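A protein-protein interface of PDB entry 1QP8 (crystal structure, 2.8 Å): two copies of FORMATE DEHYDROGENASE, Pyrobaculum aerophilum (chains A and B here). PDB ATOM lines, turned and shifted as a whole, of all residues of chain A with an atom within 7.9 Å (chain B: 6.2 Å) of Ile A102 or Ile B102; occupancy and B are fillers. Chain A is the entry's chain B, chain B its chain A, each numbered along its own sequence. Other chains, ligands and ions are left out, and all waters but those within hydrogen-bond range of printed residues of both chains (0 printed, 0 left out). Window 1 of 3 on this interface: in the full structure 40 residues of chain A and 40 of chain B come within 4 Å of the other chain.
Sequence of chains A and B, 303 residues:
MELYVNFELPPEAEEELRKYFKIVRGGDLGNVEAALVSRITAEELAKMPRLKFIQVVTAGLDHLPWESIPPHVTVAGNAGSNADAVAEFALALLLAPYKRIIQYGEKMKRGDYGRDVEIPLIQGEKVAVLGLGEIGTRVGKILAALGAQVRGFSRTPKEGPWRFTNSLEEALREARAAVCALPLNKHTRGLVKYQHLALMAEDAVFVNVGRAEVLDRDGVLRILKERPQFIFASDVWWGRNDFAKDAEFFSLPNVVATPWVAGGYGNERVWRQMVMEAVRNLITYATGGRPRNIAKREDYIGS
The backbone carbonyl oxygen of Ala A96 lies within hydrogen-bond range of the backbone NH of Ile A101, at 2.9 Å.
N of Ile B101 sits at hydrogen-bond distance from O of Ala B96 (2.9 Å).
The backbone carbonyl oxygen of Ala A96 sits at hydrogen-bond distance from the backbone NH of Ile A102, at 3.3 Å.
The backbone carbonyl oxygen (O) of Ala B96 is in hydrogen-bond range of the backbone NH (N) of Ile B102 (3.2 Å).
Among the printed residues, merely in contact across the chains: Ala A92 with Leu B95, Ala A92 with Lys B99, Ala A92 with Ile B101, Leu A93 with Ile B101, Ile A101 with Val B256, Ile A102 with Ile B102, Val A256 with Ile B101, Ala A257 with Tyr B104 and Ala A257 with Gly B105.
Of the printed residues of chain B, Ile A102 touches Ile B102 (3.8 Å).
Gly A105 touches none of the printed residues of chain B.
Met A108 touches none of the printed residues of chain B.
Printed residues of chain A within 4 Å of Leu B95: Ala A92 (3.5 Å).
Printed residues of chain A within 4 Å of Lys B99: Ala A92 (3.6 Å).
Of chain A, only Ile A102 (3.8 Å) comes within 4 Å of Ile B102.
Of the printed residues of chain A, Gly B105 touches Ala A257.
The nearest printed residue of chain B that does not touch Ile A101 is Ala B96 (4.03 Å).
Along chain A the printed residues that touch a printed residue of chain B span positions 92 to 257.
Ile A101 touches Val B256, and with the chains exchanged Val A256 touches Ile B101.
Ile A102 touches its own counterpart, Ile B102.
Positions printed for both chains: 95, 96, 97, 99, 100, 101, 102, 103, 104, 105, 106, 107 and 256.
Of the 9 pairs that touch across the chains among the printed residues, 3 have their exchanged pair printed and touching as well.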
ATOM      1  N   ALA A  92       7.955  23.108  23.543  1.00  0.00           N
ATOM      2  CA  ALA A  92       7.514  23.677  22.273  1.00  0.00           C
ATOM      3  C   ALA A  92       6.095  24.193  22.457  1.00  0.00           C
ATOM      4  O   ALA A  92       5.755  25.296  22.058  1.00  0.00           O
ATOM      5  CB  ALA A  92       7.570  22.626  21.164  1.00  0.00           C
ATOM      6  N   LEU A  93       5.279  23.396  23.106  1.00  0.00           N
ATOM      7  CA  LEU A  93       3.904  23.766  23.350  1.00  0.00           C
ATOM      8  C   LEU A  93       3.841  25.073  24.141  1.00  0.00           C
ATOM      9  O   LEU A  93       2.879  25.834  24.033  1.00  0.00           O
ATOM     10  CB  LEU A  93       3.231  22.626  24.114  1.00  0.00           C
ATOM     11  CG  LEU A  93       1.742  22.401  23.925  1.00  0.00           C
ATOM     12  CD1 LEU A  93       1.343  22.740  22.505  1.00  0.00           C
ATOM     13  CD2 LEU A  93       1.422  20.950  24.248  1.00  0.00           C
ATOM     14  N   LEU A  94       4.875  25.340  24.934  1.00  0.00           N
ATOM     15  CA  LEU A  94       4.910  26.557  25.729  1.00  0.00           C
ATOM     16  C   LEU A  94       5.490  27.731  24.975  1.00  0.00           C
ATOM     17  O   LEU A  94       4.868  28.785  24.884  1.00  0.00           O
ATOM     18  CB  LEU A  94       5.716  26.354  27.009  1.00  0.00           C
ATOM     19  CG  LEU A  94       6.150  27.651  27.708  1.00  0.00           C
ATOM     20  CD1 LEU A  94       4.954  28.411  28.260  1.00  0.00           C
ATOM     21  CD2 LEU A  94       7.100  27.304  28.822  1.00  0.00           C
ATOM     22  N   LEU A  95       6.682  27.563  24.432  1.00  0.00           N
ATOM     23  CA  LEU A  95       7.313  28.657  23.712  1.00  0.00           C
ATOM     24  C   LEU A  95       6.596  29.139  22.453  1.00  0.00           C
ATOM     25  O   LEU A  95       6.649  30.327  22.145  1.00  0.00           O
ATOM     26  CB  LEU A  95       8.749  28.295  23.355  1.00  0.00           C
ATOM     27  CG  LEU A  95       9.603  27.722  24.483  1.00  0.00           C
ATOM     28  CD1 LEU A  95      11.022  27.653  23.975  1.00  0.00           C
ATOM     29  CD2 LEU A  95       9.527  28.576  25.742  1.00  0.00           C
ATOM     30  N   ALA A  96       5.935  28.240  21.724  1.00  0.00           N
ATOM     31  CA  ALA A  96       5.246  28.635  20.497  1.00  0.00           C
ATOM     32  C   ALA A  96       4.301  29.794  20.752  1.00  0.00           C
ATOM     33  O   ALA A  96       4.370  30.818  20.069  1.00  0.00           O
ATOM     34  CB  ALA A  96       4.484  27.460  19.910  1.00  0.00           C
ATOM     35  N   PRO A  97       3.384  29.638  21.717  1.00  0.00           N
ATOM     36  CA  PRO A  97       2.461  30.730  22.003  1.00  0.00           C
ATOM     37  C   PRO A  97       3.088  31.758  22.934  1.00  0.00           C
ATOM     38  O   PRO A  97       2.809  32.947  22.829  1.00  0.00           O
ATOM     39  CB  PRO A  97       1.273  30.016  22.632  1.00  0.00           C
ATOM     40  CG  PRO A  97       1.920  28.864  23.341  1.00  0.00           C
ATOM     41  CD  PRO A  97       2.912  28.381  22.332  1.00  0.00           C
ATOM     42  N   TYR A  98       3.944  31.308  23.842  1.00  0.00           N
ATOM     43  CA  TYR A  98       4.579  32.230  24.791  1.00  0.00           C
ATOM     44  C   TYR A  98       5.417  33.305  24.106  1.00  0.00           C
ATOM     45  O   TYR A  98       5.203  34.487  24.317  1.00  0.00           O
ATOM     46  CB  TYR A  98       5.471  31.474  25.772  1.00  0.00           C
ATOM     47  CG  TYR A  98       5.870  32.290  26.984  1.00  0.00           C
ATOM     48  CD1 TYR A  98       5.005  32.424  28.080  1.00  0.00           C
ATOM     49  CD2 TYR A  98       7.106  32.921  27.042  1.00  0.00           C
ATOM     50  CE1 TYR A  98       5.370  33.160  29.196  1.00  0.00           C
ATOM     51  CE2 TYR A  98       7.479  33.667  28.151  1.00  0.00           C
ATOM     52  CZ  TYR A  98       6.609  33.781  29.222  1.00  0.00           C
ATOM     53  OH  TYR A  98       6.982  34.540  30.313  1.00  0.00           O
ATOM     54  N   LYS A  99       6.389  32.899  23.298  1.00  0.00           N
ATOM     55  CA  LYS A  99       7.217  33.885  22.625  1.00  0.00           C
ATOM     56  C   LYS A  99       6.473  34.488  21.443  1.00  0.00           C
ATOM     57  O   LYS A  99       7.065  35.167  20.603  1.00  0.00           O
ATOM     58  CB  LYS A  99       8.548  33.274  22.178  1.00  0.00           C
ATOM     59  CG  LYS A  99       9.391  32.725  23.334  1.00  0.00           C
ATOM     60  CD  LYS A  99       9.817  33.792  24.348  1.00  0.00           C
ATOM     61  CE  LYS A  99      10.764  34.804  23.725  1.00  0.00           C
ATOM     62  NZ  LYS A  99      11.330  35.777  24.708  1.00  0.00           N
ATOM     63  N   ARG A 100       5.165  34.238  21.401  1.00  0.00           N
ATOM     64  CA  ARG A 100       4.274  34.764  20.364  1.00  0.00           C
ATOM     65  C   ARG A 100       4.691  34.379  18.939  1.00  0.00           C
ATOM     66  O   ARG A 100       4.448  35.123  17.996  1.00  0.00           O
ATOM     67  CB  ARG A 100       4.208  36.292  20.453  1.00  0.00           C
ATOM     68  CG  ARG A 100       4.315  36.893  21.846  1.00  0.00           C
ATOM     69  CD  ARG A 100       2.974  37.252  22.466  1.00  0.00           C
ATOM     70  NE  ARG A 100       2.414  36.145  23.231  1.00  0.00           N
ATOM     71  CZ  ARG A 100       1.978  36.239  24.488  1.00  0.00           C
ATOM     72  NH1 ARG A 100       2.031  37.400  25.134  1.00  0.00           N
ATOM     73  NH2 ARG A 100       1.492  35.169  25.106  1.00  0.00           N
ATOM     74  N   ILE A 101       5.319  33.224  18.775  1.00  0.00           N
ATOM     75  CA  ILE A 101       5.739  32.800  17.446  1.00  0.00           C
ATOM     76  C   ILE A 101       4.512  32.555  16.555  1.00  0.00           C
ATOM     77  O   ILE A 101       4.408  33.088  15.446  1.00  0.00           O
ATOM     78  CB  ILE A 101       6.579  31.489  17.518  1.00  0.00           C
ATOM     79  CG1 ILE A 101       7.763  31.668  18.486  1.00  0.00           C
ATOM     80  CG2 ILE A 101       7.040  31.074  16.115  1.00  0.00           C
ATOM     81  CD1 ILE A 101       8.678  32.821  18.168  1.00  0.00           C
ATOM     82  N   ILE A 102       3.578  31.745  17.041  1.00  0.00           N
ATOM     83  CA  ILE A 102       2.393  31.432  16.259  1.00  0.00           C
ATOM     84  C   ILE A 102       1.640  32.686  15.864  1.00  0.00           C
ATOM     85  O   ILE A 102       1.289  32.858  14.696  1.00  0.00           O
ATOM     86  CB  ILE A 102       1.444  30.525  17.027  1.00  0.00           C
ATOM     87  CG1 ILE A 102       2.113  29.182  17.296  1.00  0.00           C
ATOM     88  CG2 ILE A 102       0.203  30.283  16.226  1.00  0.00           C
ATOM     89  CD1 ILE A 102       1.278  28.263  18.189  1.00  0.00           C
ATOM     90  N   GLN A 103       1.402  33.558  16.843  1.00  0.00           N
ATOM     91  CA  GLN A 103       0.683  34.812  16.626  1.00  0.00           C
ATOM     92  C   GLN A 103       1.336  35.688  15.565  1.00  0.00           C
ATOM     93  O   GLN A 103       0.700  36.053  14.582  1.00  0.00           O
ATOM     94  CB  GLN A 103       0.566  35.601  17.940  1.00  0.00           C
ATOM     95  CG  GLN A 103      -0.198  34.866  19.051  1.00  0.00           C
ATOM     96  CD  GLN A 103       0.712  34.038  19.975  1.00  0.00           C
ATOM     97  OE1 GLN A 103       1.706  33.427  19.527  1.00  0.00           O
ATOM     98  NE2 GLN A 103       0.366  34.003  21.270  1.00  0.00           N
ATOM     99  N   TYR A 104       2.603  36.033  15.753  1.00  0.00           N
ATOM    100  CA  TYR A 104       3.281  36.872  14.773  1.00  0.00           C
ATOM    101  C   TYR A 104       3.381  36.215  13.405  1.00  0.00           C
ATOM    102  O   TYR A 104       3.309  36.898  12.392  1.00  0.00           O
ATOM    103  CB  TYR A 104       4.677  37.261  15.256  1.00  0.00           C
ATOM    104  CG  TYR A 104       4.706  38.589  15.986  1.00  0.00           C
ATOM    105  CD1 TYR A 104       4.964  38.650  17.354  1.00  0.00           C
ATOM    106  CD2 TYR A 104       4.452  39.781  15.305  1.00  0.00           C
ATOM    107  CE1 TYR A 104       4.968  39.861  18.027  1.00  0.00           C
ATOM    108  CE2 TYR A 104       4.449  40.992  15.962  1.00  0.00           C
ATOM    109  CZ  TYR A 104       4.708  41.032  17.327  1.00  0.00           C
ATOM    110  OH  TYR A 104       4.694  42.242  17.995  1.00  0.00           O
ATOM    111  N   GLY A 105       3.545  34.897  13.368  1.00  0.00           N
ATOM    112  CA  GLY A 105       3.630  34.222  12.091  1.00  0.00           C
ATOM    113  C   GLY A 105       2.341  34.441  11.316  1.00  0.00           C
ATOM    114  O   GLY A 105       2.340  34.537  10.083  1.00  0.00           O
ATOM    115  N   GLU A 106       1.228  34.511  12.042  1.00  0.00           N
ATOM    116  CA  GLU A 106      -0.055  34.735  11.406  1.00  0.00           C
ATOM    117  C   GLU A 106      -0.114  36.157  10.863  1.00  0.00           C
ATOM    118  O   GLU A 106      -0.472  36.371   9.705  1.00  0.00           O
ATOM    119  CB  GLU A 106      -1.184  34.497  12.401  1.00  0.00           C
ATOM    120  CG  GLU A 106      -1.638  33.067  12.398  1.00  0.00           C
ATOM    121  CD  GLU A 106      -1.876  32.577  10.983  1.00  0.00           C
ATOM    122  OE1 GLU A 106      -2.643  33.246  10.248  1.00  0.00           O
ATOM    123  OE2 GLU A 106      -1.294  31.535  10.603  1.00  0.00           O
ATOM    124  N   LYS A 107       0.265  37.119  11.698  1.00  0.00           N
ATOM    125  CA  LYS A 107       0.239  38.507  11.298  1.00  0.00           C
ATOM    126  C   LYS A 107       1.095  38.723  10.060  1.00  0.00           C
ATOM    127  O   LYS A 107       0.717  39.490   9.173  1.00  0.00           O
ATOM    128  CB  LYS A 107       0.722  39.394  12.436  1.00  0.00           C
ATOM    129  CG  LYS A 107      -0.155  39.341  13.670  1.00  0.00           C
ATOM    130  CD  LYS A 107       0.455  40.143  14.816  1.00  0.00           C
ATOM    131  CE  LYS A 107       0.613  41.619  14.430  1.00  0.00           C
ATOM    132  NZ  LYS A 107       1.566  42.395  15.302  1.00  0.00           N
ATOM    133  N   MET A 108       2.238  38.045   9.990  1.00  0.00           N
ATOM    134  CA  MET A 108       3.114  38.184   8.830  1.00  0.00           C
ATOM    135  C   MET A 108       2.401  37.682   7.586  1.00  0.00           C
ATOM    136  O   MET A 108       2.397  38.332   6.543  1.00  0.00           O
ATOM    137  CB  MET A 108       4.402  37.383   9.014  1.00  0.00           C
ATOM    138  CG  MET A 108       5.306  37.902  10.099  1.00  0.00           C
ATOM    139  SD  MET A 108       5.891  39.587   9.803  1.00  0.00           S
ATOM    140  CE  MET A 108       7.423  39.274   8.872  1.00  0.00           C
ATOM    141  N   LYS A 109       1.798  36.511   7.705  1.00  0.00           N
ATOM    142  CA  LYS A 109       1.100  35.920   6.580  1.00  0.00           C
ATOM    143  C   LYS A 109      -0.014  36.814   6.046  1.00  0.00           C
ATOM    144  O   LYS A 109      -0.242  36.860   4.849  1.00  0.00           O
ATOM    145  CB  LYS A 109       0.497  34.567   6.975  1.00  0.00           C
ATOM    146  CG  LYS A 109       1.442  33.382   7.021  1.00  0.00           C
ATOM    147  CD  LYS A 109       0.609  32.108   7.130  1.00  0.00           C
ATOM    148  CE  LYS A 109       1.438  30.827   7.258  1.00  0.00           C
ATOM    149  NZ  LYS A 109       1.625  30.371   8.694  1.00  0.00           N
ATOM    150  N   ILE A 231      -3.848  31.814  27.366  1.00  0.00           N
ATOM    151  CA  ILE A 231      -3.746  30.773  26.362  1.00  0.00           C
ATOM    152  C   ILE A 231      -3.691  29.376  26.928  1.00  0.00           C
ATOM    153  O   ILE A 231      -2.972  29.106  27.871  1.00  0.00           O
ATOM    154  CB  ILE A 231      -2.486  30.984  25.507  1.00  0.00           C
ATOM    155  CG1 ILE A 231      -2.516  32.374  24.888  1.00  0.00           C
ATOM    156  CG2 ILE A 231      -2.398  29.934  24.431  1.00  0.00           C
ATOM    157  CD1 ILE A 231      -1.276  32.688  24.110  1.00  0.00           C
ATOM    158  N   ALA A 233      -2.722  25.675  25.828  1.00  0.00           N
ATOM    159  CA  ALA A 233      -2.047  24.865  24.821  1.00  0.00           C
ATOM    160  C   ALA A 233      -1.997  23.445  25.357  1.00  0.00           C
ATOM    161  O   ALA A 233      -1.292  23.168  26.335  1.00  0.00           O
ATOM    162  CB  ALA A 233      -0.652  25.377  24.605  1.00  0.00           C
ATOM    163  N   PRO A 253      -9.604  31.391  19.623  1.00  0.00           N
ATOM    164  CA  PRO A 253      -8.346  31.970  19.148  1.00  0.00           C
ATOM    165  C   PRO A 253      -7.211  31.797  20.129  1.00  0.00           C
ATOM    166  O   PRO A 253      -6.051  31.786  19.734  1.00  0.00           O
ATOM    167  CB  PRO A 253      -8.659  33.467  19.002  1.00  0.00           C
ATOM    168  CG  PRO A 253     -10.130  33.592  19.214  1.00  0.00           C
ATOM    169  CD  PRO A 253     -10.501  32.441  20.114  1.00  0.00           C
ATOM    170  N   VAL A 255      -6.381  29.208  21.955  1.00  0.00           N
ATOM    171  CA  VAL A 255      -6.135  27.807  22.248  1.00  0.00           C
ATOM    172  C   VAL A 255      -5.181  27.207  21.217  1.00  0.00           C
ATOM    173  O   VAL A 255      -5.302  27.492  20.024  1.00  0.00           O
ATOM    174  CB  VAL A 255      -7.445  27.004  22.220  1.00  0.00           C
ATOM    175  CG1 VAL A 255      -7.180  25.536  22.550  1.00  0.00           C
ATOM    176  CG2 VAL A 255      -8.414  27.600  23.214  1.00  0.00           C
ATOM    177  N   VAL A 256      -4.207  26.423  21.684  1.00  0.00           N
ATOM    178  CA  VAL A 256      -3.263  25.738  20.797  1.00  0.00           C
ATOM    179  C   VAL A 256      -3.546  24.295  21.105  1.00  0.00           C
ATOM    180  O   VAL A 256      -3.509  23.900  22.265  1.00  0.00           O
ATOM    181  CB  VAL A 256      -1.785  25.977  21.149  1.00  0.00           C
ATOM    182  CG1 VAL A 256      -0.896  25.249  20.137  1.00  0.00           C
ATOM    183  CG2 VAL A 256      -1.476  27.475  21.185  1.00  0.00           C
ATOM    184  N   ALA A 257      -3.801  23.498  20.081  1.00  0.00           N
ATOM    185  CA  ALA A 257      -4.157  22.117  20.305  1.00  0.00           C
ATOM    186  C   ALA A 257      -3.441  21.119  19.413  1.00  0.00           C
ATOM    187  O   ALA A 257      -3.300  21.325  18.208  1.00  0.00           O
ATOM    188  CB  ALA A 257      -5.649  21.984  20.131  1.00  0.00           C
ATOM    189  N   THR A 258      -2.989  20.032  20.023  1.00  0.00           N
ATOM    190  CA  THR A 258      -2.299  18.966  19.310  1.00  0.00           C
ATOM    191  C   THR A 258      -3.025  17.669  19.665  1.00  0.00           C
ATOM    192  O   THR A 258      -3.513  17.516  20.790  1.00  0.00           O
ATOM    193  CB  THR A 258      -0.804  18.900  19.714  1.00  0.00           C
ATOM    194  OG1 THR A 258      -0.680  18.952  21.138  1.00  0.00           O
ATOM    195  CG2 THR A 258      -0.047  20.062  19.112  1.00  0.00           C
ATOM    196  N   LEU B  95      11.537  25.142  17.995  1.00  0.00           N
ATOM    197  CA  LEU B  95      10.584  24.151  18.456  1.00  0.00           C
ATOM    198  C   LEU B  95       9.167  24.258  17.881  1.00  0.00           C
ATOM    199  O   LEU B  95       8.505  23.242  17.703  1.00  0.00           O
ATOM    200  CB  LEU B  95      10.509  24.182  19.990  1.00  0.00           C
ATOM    201  CG  LEU B  95      11.813  24.072  20.790  1.00  0.00           C
ATOM    202  CD1 LEU B  95      11.498  23.986  22.268  1.00  0.00           C
ATOM    203  CD2 LEU B  95      12.566  22.850  20.352  1.00  0.00           C
ATOM    204  N   ALA B  96       8.692  25.470  17.599  1.00  0.00           N
ATOM    205  CA  ALA B  96       7.336  25.633  17.076  1.00  0.00           C
ATOM    206  C   ALA B  96       7.131  24.812  15.820  1.00  0.00           C
ATOM    207  O   ALA B  96       6.173  24.045  15.724  1.00  0.00           O
ATOM    208  CB  ALA B  96       7.029  27.099  16.799  1.00  0.00           C
ATOM    209  N   PRO B  97       8.015  24.978  14.824  1.00  0.00           N
ATOM    210  CA  PRO B  97       7.891  24.212  13.582  1.00  0.00           C
ATOM    211  C   PRO B  97       8.479  22.808  13.748  1.00  0.00           C
ATOM    212  O   PRO B  97       7.948  21.830  13.209  1.00  0.00           O
ATOM    213  CB  PRO B  97       8.710  25.018  12.562  1.00  0.00           C
ATOM    214  CG  PRO B  97       9.176  26.261  13.297  1.00  0.00           C
ATOM    215  CD  PRO B  97       9.122  25.948  14.751  1.00  0.00           C
ATOM    216  N   LYS B  99       8.831  20.663  16.498  1.00  0.00           N
ATOM    217  CA  LYS B  99       7.962  19.686  17.137  1.00  0.00           C
ATOM    218  C   LYS B  99       6.580  19.672  16.476  1.00  0.00           C
ATOM    219  O   LYS B  99       5.623  19.084  17.008  1.00  0.00           O
ATOM    220  CB  LYS B  99       7.847  19.977  18.639  1.00  0.00           C
ATOM    221  CG  LYS B  99       9.180  19.983  19.364  1.00  0.00           C
ATOM    222  CD  LYS B  99       9.826  18.616  19.385  1.00  0.00           C
ATOM    223  CE  LYS B  99       9.241  17.742  20.483  1.00  0.00           C
ATOM    224  NZ  LYS B  99       9.737  16.328  20.405  1.00  0.00           N
ATOM    225  N   ARG B 100       6.491  20.334  15.321  1.00  0.00           N
ATOM    226  CA  ARG B 100       5.257  20.388  14.540  1.00  0.00           C
ATOM    227  C   ARG B 100       4.057  20.988  15.294  1.00  0.00           C
ATOM    228  O   ARG B 100       2.901  20.641  15.020  1.00  0.00           O
ATOM    229  CB  ARG B 100       4.915  18.971  14.078  1.00  0.00           C
ATOM    230  CG  ARG B 100       6.136  18.120  13.678  1.00  0.00           C
ATOM    231  CD  ARG B 100       6.494  18.219  12.199  1.00  0.00           C
ATOM    232  NE  ARG B 100       7.812  18.798  11.961  1.00  0.00           N
ATOM    233  CZ  ARG B 100       8.741  18.241  11.183  1.00  0.00           C
ATOM    234  NH1 ARG B 100       8.500  17.079  10.572  1.00  0.00           N
ATOM    235  NH2 ARG B 100       9.907  18.850  10.986  1.00  0.00           N
ATOM    236  N   ILE B 101       4.318  21.879  16.245  1.00  0.00           N
ATOM    237  CA  ILE B 101       3.227  22.491  16.995  1.00  0.00           C
ATOM    238  C   ILE B 101       2.334  23.340  16.077  1.00  0.00           C
ATOM    239  O   ILE B 101       1.104  23.184  16.059  1.00  0.00           O
ATOM    240  CB  ILE B 101       3.755  23.406  18.112  1.00  0.00           C
ATOM    241  CG1 ILE B 101       4.578  22.598  19.124  1.00  0.00           C
ATOM    242  CG2 ILE B 101       2.590  24.094  18.799  1.00  0.00           C
ATOM    243  CD1 ILE B 101       3.758  21.651  19.976  1.00  0.00           C
ATOM    244  N   ILE B 102       2.959  24.242  15.318  1.00  0.00           N
ATOM    245  CA  ILE B 102       2.206  25.105  14.421  1.00  0.00           C
ATOM    246  C   ILE B 102       1.374  24.307  13.440  1.00  0.00           C
ATOM    247  O   ILE B 102       0.187  24.582  13.256  1.00  0.00           O
ATOM    248  CB  ILE B 102       3.113  26.008  13.600  1.00  0.00           C
ATOM    249  CG1 ILE B 102       3.682  27.131  14.459  1.00  0.00           C
ATOM    250  CG2 ILE B 102       2.319  26.624  12.473  1.00  0.00           C
ATOM    251  CD1 ILE B 102       4.642  28.016  13.698  1.00  0.00           C
ATOM    252  N   GLN B 103       2.002  23.330  12.798  1.00  0.00           N
ATOM    253  CA  GLN B 103       1.297  22.513  11.813  1.00  0.00           C
ATOM    254  C   GLN B 103       0.123  21.730  12.401  1.00  0.00           C
ATOM    255  O   GLN B 103      -0.988  21.801  11.878  1.00  0.00           O
ATOM    256  CB  GLN B 103       2.266  21.580  11.064  1.00  0.00           C
ATOM    257  CG  GLN B 103       3.506  21.180  11.825  1.00  0.00           C
ATOM    258  CD  GLN B 103       4.612  22.238  11.810  1.00  0.00           C
ATOM    259  OE1 GLN B 103       5.567  22.154  11.032  1.00  0.00           O
ATOM    260  NE2 GLN B 103       4.486  23.233  12.683  1.00  0.00           N
ATOM    261  N   TYR B 104       0.337  21.006  13.494  1.00  0.00           N
ATOM    262  CA  TYR B 104      -0.778  20.263  14.074  1.00  0.00           C
ATOM    263  C   TYR B 104      -1.875  21.190  14.601  1.00  0.00           C
ATOM    264  O   TYR B 104      -3.056  20.858  14.554  1.00  0.00           O
ATOM    265  CB  TYR B 104      -0.291  19.321  15.183  1.00  0.00           C
ATOM    266  CG  TYR B 104      -0.005  17.911  14.694  1.00  0.00           C
ATOM    267  CD1 TYR B 104       1.296  17.403  14.669  1.00  0.00           C
ATOM    268  CD2 TYR B 104      -1.035  17.089  14.248  1.00  0.00           C
ATOM    269  CE1 TYR B 104       1.570  16.105  14.206  1.00  0.00           C
ATOM    270  CE2 TYR B 104      -0.774  15.784  13.786  1.00  0.00           C
ATOM    271  CZ  TYR B 104       0.533  15.300  13.767  1.00  0.00           C
ATOM    272  OH  TYR B 104       0.788  14.029  13.302  1.00  0.00           O
ATOM    273  N   GLY B 105      -1.487  22.360  15.093  1.00  0.00           N
ATOM    274  CA  GLY B 105      -2.482  23.288  15.595  1.00  0.00           C
ATOM    275  C   GLY B 105      -3.420  23.676  14.468  1.00  0.00           C
ATOM    276  O   GLY B 105      -4.622  23.860  14.677  1.00  0.00           O
ATOM    277  N   GLU B 106      -2.864  23.800  13.262  1.00  0.00           N
ATOM    278  CA  GLU B 106      -3.656  24.153  12.094  1.00  0.00           C
ATOM    279  C   GLU B 106      -4.599  23.015  11.770  1.00  0.00           C
ATOM    280  O   GLU B 106      -5.799  23.224  11.590  1.00  0.00           O
ATOM    281  CB  GLU B 106      -2.768  24.437  10.880  1.00  0.00           C
ATOM    282  CG  GLU B 106      -1.958  25.714  10.984  1.00  0.00           C
ATOM    283  CD  GLU B 106      -2.774  26.872  11.525  1.00  0.00           C
ATOM    284  OE1 GLU B 106      -3.876  27.129  10.998  1.00  0.00           O
ATOM    285  OE2 GLU B 106      -2.314  27.532  12.483  1.00  0.00           O
ATOM    286  N   LYS B 107      -4.062  21.800  11.713  1.00  0.00           N
ATOM    287  CA  LYS B 107      -4.889  20.644  11.398  1.00  0.00           C
ATOM    288  C   LYS B 107      -6.035  20.499  12.386  1.00  0.00           C
ATOM    289  O   LYS B 107      -7.145  20.159  11.993  1.00  0.00           O
ATOM    290  CB  LYS B 107      -4.036  19.385  11.363  1.00  0.00           C
ATOM    291  CG  LYS B 107      -2.835  19.539  10.418  1.00  0.00           C
ATOM    292  CD  LYS B 107      -1.967  18.290  10.359  1.00  0.00           C
ATOM    293  CE  LYS B 107      -2.788  17.104   9.903  1.00  0.00           C
ATOM    294  NZ  LYS B 107      -1.939  15.975   9.499  1.00  0.00           N
ATOM    295  N   VAL B 256       8.250  30.313   8.513  1.00  0.00           N
ATOM    296  CA  VAL B 256       7.685  30.872   9.728  1.00  0.00           C
ATOM    297  C   VAL B 256       8.409  32.190   9.811  1.00  0.00           C
ATOM    298  O   VAL B 256       9.636  32.234   9.732  1.00  0.00           O
ATOM    299  CB  VAL B 256       8.023  30.072  10.985  1.00  0.00           C
ATOM    300  CG1 VAL B 256       7.655  30.903  12.214  1.00  0.00           C
ATOM    301  CG2 VAL B 256       7.250  28.729  10.996  1.00  0.00           C
